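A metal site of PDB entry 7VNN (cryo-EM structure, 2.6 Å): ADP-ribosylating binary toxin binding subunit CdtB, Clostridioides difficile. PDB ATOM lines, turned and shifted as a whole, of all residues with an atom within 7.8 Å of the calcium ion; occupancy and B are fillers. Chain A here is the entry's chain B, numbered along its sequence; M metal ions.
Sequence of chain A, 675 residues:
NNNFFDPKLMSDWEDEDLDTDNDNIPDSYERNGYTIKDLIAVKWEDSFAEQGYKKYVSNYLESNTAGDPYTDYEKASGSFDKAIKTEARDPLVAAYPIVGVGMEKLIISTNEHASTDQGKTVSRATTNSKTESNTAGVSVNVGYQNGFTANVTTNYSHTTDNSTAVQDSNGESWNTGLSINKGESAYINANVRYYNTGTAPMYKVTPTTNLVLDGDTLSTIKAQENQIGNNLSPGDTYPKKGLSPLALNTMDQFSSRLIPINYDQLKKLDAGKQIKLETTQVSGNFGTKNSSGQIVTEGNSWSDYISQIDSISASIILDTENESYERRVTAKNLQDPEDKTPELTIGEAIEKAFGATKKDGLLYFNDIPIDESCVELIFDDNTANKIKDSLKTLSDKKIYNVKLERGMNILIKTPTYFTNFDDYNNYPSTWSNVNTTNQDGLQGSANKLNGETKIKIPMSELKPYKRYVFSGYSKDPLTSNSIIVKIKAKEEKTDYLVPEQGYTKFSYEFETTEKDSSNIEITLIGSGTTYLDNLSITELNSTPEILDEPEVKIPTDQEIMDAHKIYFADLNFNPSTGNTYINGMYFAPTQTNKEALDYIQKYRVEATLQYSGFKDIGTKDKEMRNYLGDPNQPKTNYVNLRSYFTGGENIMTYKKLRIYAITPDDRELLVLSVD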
ATOM      1  N   SER A 373      16.025  30.262  -4.828  1.00  0.00           N
ATOM      2  CA  SER A 373      15.624  29.403  -3.711  1.00  0.00           C
ATOM      3  C   SER A 373      16.786  29.037  -2.803  1.00  0.00           C
ATOM      4  O   SER A 373      16.550  28.470  -1.730  1.00  0.00           O
ATOM      5  CB  SER A 373      14.973  28.132  -4.247  1.00  0.00           C
ATOM      6  OG  SER A 373      15.907  27.328  -4.948  1.00  0.00           O
ATOM      7  N   PHE A 418      24.557  25.656   3.688  1.00  0.00           N
ATOM      8  CA  PHE A 418      23.363  25.413   2.897  1.00  0.00           C
ATOM      9  C   PHE A 418      23.279  23.934   2.561  1.00  0.00           C
ATOM     10  O   PHE A 418      24.310  23.246   2.432  1.00  0.00           O
ATOM     11  CB  PHE A 418      23.360  26.250   1.616  1.00  0.00           C
ATOM     12  CG  PHE A 418      22.247  25.919   0.663  1.00  0.00           C
ATOM     13  CD1 PHE A 418      20.960  26.370   0.914  1.00  0.00           C
ATOM     14  CD2 PHE A 418      22.483  25.194  -0.484  1.00  0.00           C
ATOM     15  CE1 PHE A 418      19.939  26.074   0.039  1.00  0.00           C
ATOM     16  CE2 PHE A 418      21.462  24.898  -1.360  1.00  0.00           C
ATOM     17  CZ  PHE A 418      20.185  25.339  -1.098  1.00  0.00           C
ATOM     18  N   THR A 419      22.054  23.435   2.430  1.00  0.00           N
ATOM     19  CA  THR A 419      21.830  22.059   2.012  1.00  0.00           C
ATOM     20  C   THR A 419      20.516  21.979   1.247  1.00  0.00           C
ATOM     21  O   THR A 419      19.571  22.716   1.535  1.00  0.00           O
ATOM     22  CB  THR A 419      21.790  21.103   3.217  1.00  0.00           C
ATOM     23  OG1 THR A 419      21.480  19.778   2.762  1.00  0.00           O
ATOM     24  CG2 THR A 419      20.738  21.543   4.222  1.00  0.00           C
ATOM     25  N   ASN A 420      20.483  21.105   0.254  1.00  0.00           N
ATOM     26  CA  ASN A 420      19.271  20.813  -0.499  1.00  0.00           C
ATOM     27  C   ASN A 420      18.970  19.331  -0.581  1.00  0.00           C
ATOM     28  O   ASN A 420      17.971  18.946  -1.197  1.00  0.00           O
ATOM     29  CB  ASN A 420      19.351  21.399  -1.914  1.00  0.00           C
ATOM     30  CG  ASN A 420      20.614  20.983  -2.641  1.00  0.00           C
ATOM     31  OD1 ASN A 420      21.517  20.391  -2.044  1.00  0.00           O
ATOM     32  ND2 ASN A 420      20.690  21.290  -3.921  1.00  0.00           N
ATOM     33  N   PHE A 421      19.805  18.478   0.022  1.00  0.00           N
ATOM     34  CA  PHE A 421      19.629  17.034   0.095  1.00  0.00           C
ATOM     35  C   PHE A 421      19.684  16.360  -1.270  1.00  0.00           C
ATOM     36  O   PHE A 421      19.255  15.217  -1.421  1.00  0.00           O
ATOM     37  CB  PHE A 421      18.312  16.666   0.800  1.00  0.00           C
ATOM     38  CG  PHE A 421      17.993  17.537   1.980  1.00  0.00           C
ATOM     39  CD1 PHE A 421      18.881  17.679   3.026  1.00  0.00           C
ATOM     40  CD2 PHE A 421      16.783  18.213   2.043  1.00  0.00           C
ATOM     41  CE1 PHE A 421      18.594  18.483   4.111  1.00  0.00           C
ATOM     42  CE2 PHE A 421      16.475  19.013   3.134  1.00  0.00           C
ATOM     43  CZ  PHE A 421      17.382  19.157   4.165  1.00  0.00           C
ATOM     44  N   ASP A 422      20.210  17.050  -2.285  1.00  0.00           N
ATOM     45  CA  ASP A 422      20.368  16.471  -3.611  1.00  0.00           C
ATOM     46  C   ASP A 422      21.825  16.350  -4.021  1.00  0.00           C
ATOM     47  O   ASP A 422      22.296  15.243  -4.300  1.00  0.00           O
ATOM     48  CB  ASP A 422      19.590  17.288  -4.647  1.00  0.00           C
ATOM     49  CG  ASP A 422      18.148  17.481  -4.268  1.00  0.00           C
ATOM     50  OD1 ASP A 422      17.428  16.468  -4.204  1.00  0.00           O
ATOM     51  OD2 ASP A 422      17.735  18.630  -4.022  1.00  0.00           O
ATOM     52  N   ASP A 423      22.562  17.460  -4.071  1.00  0.00           N
ATOM     53  CA  ASP A 423      23.963  17.433  -4.462  1.00  0.00           C
ATOM     54  C   ASP A 423      24.852  18.361  -3.646  1.00  0.00           C
ATOM     55  O   ASP A 423      26.076  18.205  -3.706  1.00  0.00           O
ATOM     56  CB  ASP A 423      24.101  17.803  -5.949  1.00  0.00           C
ATOM     57  CG  ASP A 423      23.304  19.037  -6.320  1.00  0.00           C
ATOM     58  OD1 ASP A 423      22.553  19.546  -5.466  1.00  0.00           O
ATOM     59  OD2 ASP A 423      23.441  19.506  -7.474  1.00  0.00           O
ATOM     60  N   ASP A 440      10.499  14.630  -3.983  1.00  0.00           N
ATOM     61  CA  ASP A 440       9.637  15.701  -3.511  1.00  0.00           C
ATOM     62  C   ASP A 440      10.479  16.900  -3.111  1.00  0.00           C
ATOM     63  O   ASP A 440      11.681  16.929  -3.392  1.00  0.00           O
ATOM     64  CB  ASP A 440       8.773  15.231  -2.336  1.00  0.00           C
ATOM     65  CG  ASP A 440       7.429  14.685  -2.789  1.00  0.00           C
ATOM     66  OD1 ASP A 440       6.867  15.226  -3.768  1.00  0.00           O
ATOM     67  OD2 ASP A 440       6.938  13.707  -2.181  1.00  0.00           O
ATOM     68  N   GLY A 441       9.879  17.881  -2.459  1.00  0.00           N
ATOM     69  CA  GLY A 441      10.599  19.107  -2.167  1.00  0.00           C
ATOM     70  C   GLY A 441      10.737  19.972  -3.389  1.00  0.00           C
ATOM     71  O   GLY A 441      10.062  19.791  -4.405  1.00  0.00           O
ATOM     72  N   LEU A 442      11.629  20.962  -3.293  1.00  0.00           N
ATOM     73  CA  LEU A 442      11.872  21.854  -4.417  1.00  0.00           C
ATOM     74  C   LEU A 442      12.381  21.090  -5.631  1.00  0.00           C
ATOM     75  O   LEU A 442      11.853  21.233  -6.737  1.00  0.00           O
ATOM     76  CB  LEU A 442      12.845  22.966  -4.032  1.00  0.00           C
ATOM     77  CG  LEU A 442      12.243  24.241  -3.432  1.00  0.00           C
ATOM     78  CD1 LEU A 442      11.313  24.901  -4.430  1.00  0.00           C
ATOM     79  CD2 LEU A 442      11.536  23.979  -2.121  1.00  0.00           C
ATOM     80  N   GLN A 443      13.414  20.249  -5.449  1.00  0.00           N
ATOM     81  CA  GLN A 443      13.917  19.390  -6.521  1.00  0.00           C
ATOM     82  C   GLN A 443      14.308  18.041  -5.914  1.00  0.00           C
ATOM     83  O   GLN A 443      15.451  17.853  -5.499  1.00  0.00           O
ATOM     84  CB  GLN A 443      15.095  20.029  -7.246  1.00  0.00           C
ATOM     85  CG  GLN A 443      14.795  21.360  -7.919  1.00  0.00           C
ATOM     86  CD  GLN A 443      15.433  22.529  -7.197  1.00  0.00           C
ATOM     87  OE1 GLN A 443      16.523  22.419  -6.632  1.00  0.00           O
ATOM     88  NE2 GLN A 443      14.754  23.671  -7.211  1.00  0.00           N
ATOM     89  N   GLY A 444      13.358  17.117  -5.868  1.00  0.00           N
ATOM     90  CA  GLY A 444      13.650  15.730  -5.536  1.00  0.00           C
ATOM     91  C   GLY A 444      14.308  15.480  -4.188  1.00  0.00           C
ATOM     92  O   GLY A 444      15.271  14.708  -4.114  1.00  0.00           O
ATOM     93  N   SER A 445      13.804  16.111  -3.131  1.00  0.00           N
ATOM     94  CA  SER A 445      14.351  15.882  -1.797  1.00  0.00           C
ATOM     95  C   SER A 445      13.358  16.364  -0.751  1.00  0.00           C
ATOM     96  O   SER A 445      12.862  17.485  -0.839  1.00  0.00           O
ATOM     97  CB  SER A 445      15.692  16.593  -1.616  1.00  0.00           C
ATOM     98  OG  SER A 445      15.560  17.997  -1.806  1.00  0.00           O
ATOM     99  N   ALA A 446      13.100  15.520   0.238  1.00  0.00           N
ATOM    100  CA  ALA A 446      12.136  15.837   1.288  1.00  0.00           C
ATOM    101  C   ALA A 446      12.774  15.972   2.659  1.00  0.00           C
ATOM    102  O   ALA A 446      12.638  17.017   3.306  1.00  0.00           O
ATOM    103  CB  ALA A 446      11.034  14.774   1.326  1.00  0.00           C
ATOM    104  N   LEU A 532      10.342  19.352   3.960  1.00  0.00           N
ATOM    105  CA  LEU A 532      11.337  20.395   4.095  1.00  0.00           C
ATOM    106  C   LEU A 532      12.244  20.383   2.875  1.00  0.00           C
ATOM    107  O   LEU A 532      12.310  19.393   2.145  1.00  0.00           O
ATOM    108  CB  LEU A 532      12.172  20.222   5.368  1.00  0.00           C
ATOM    109  CG  LEU A 532      11.498  20.455   6.717  1.00  0.00           C
ATOM    110  CD1 LEU A 532      12.463  20.136   7.853  1.00  0.00           C
ATOM    111  CD2 LEU A 532      10.985  21.878   6.841  1.00  0.00           C
ATOM    112  N   ASP A 533      12.929  21.504   2.644  1.00  0.00           N
ATOM    113  CA  ASP A 533      13.918  21.605   1.579  1.00  0.00           C
ATOM    114  C   ASP A 533      14.643  22.938   1.696  1.00  0.00           C
ATOM    115  O   ASP A 533      14.082  23.921   2.171  1.00  0.00           O
ATOM    116  CB  ASP A 533      13.270  21.479   0.197  1.00  0.00           C
ATOM    117  CG  ASP A 533      14.145  20.712  -0.785  1.00  0.00           C
ATOM    118  OD1 ASP A 533      15.304  20.424  -0.442  1.00  0.00           O
ATOM    119  OD2 ASP A 533      13.661  20.397  -1.890  1.00  0.00           O
ATOM    120  N   ASN A 534      15.908  22.937   1.252  1.00  0.00           N
ATOM    121  CA  ASN A 534      16.723  24.144   1.120  1.00  0.00           C
ATOM    122  C   ASN A 534      16.849  24.885   2.453  1.00  0.00           C
ATOM    123  O   ASN A 534      16.402  26.019   2.626  1.00  0.00           O
ATOM    124  CB  ASN A 534      16.153  25.068   0.026  1.00  0.00           C
ATOM    125  CG  ASN A 534      16.208  24.443  -1.352  1.00  0.00           C
ATOM    126  OD1 ASN A 534      16.798  23.379  -1.539  1.00  0.00           O
ATOM    127  ND2 ASN A 534      15.599  25.115  -2.322  1.00  0.00           N
HETATM  128 CA    CA M   1      15.694  19.890  -3.307  1.00  0.00          CA
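The side-chain hydroxyl (OG) of Ser 445 sits close to the backbone carbonyl oxygen (O) of Asn 420 (2.7 Å).
The side-chain carboxylate (OD1) of Asp 422 sits close to the backbone carbonyl oxygen (O) of Gln 443 (2.7 Å).
OD1 of Asn 534 lies close to OD1 of Asp 533, 3.5 Å away.
The backbone NH of Leu 442 sits close to the side-chain carboxylate of Asp 533 (2.5 Å).
The side-chain carboxylate of Asp 423 is in hydrogen-bond range of the side-chain amide nitrogen of Asn 420, at 3.0 Å.
Asn 420 touches the calcium ion.
Within 4 Å of the calcium ion: Asn 420, Asp 422, Gln 443, Ser 445 and Asp 533.
The nearest printed residue that does not touch the calcium ion is Asn 534 (4.1 Å).
OG of Ser 445 is bound to the calcium ion, 2.4 Å away.
The calcium ion is bound by the side-chain carboxylate (OD2) of Asp 422 (2.5 Å).
OD2 of Asp 533 binds the calcium ion (2.5 Å).
The calcium ion has three donor atoms within binding distance.
Slightly farther from the calcium ion lies the side-chain carboxylate (OD1) of Asp 533 (2.9 Å).
Slightly farther from the calcium ion lies the backbone carbonyl oxygen (O) of Gln 443 (3.0 Å).
Slightly farther from the calcium ion lies N of Gln 443 (3.1 Å).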
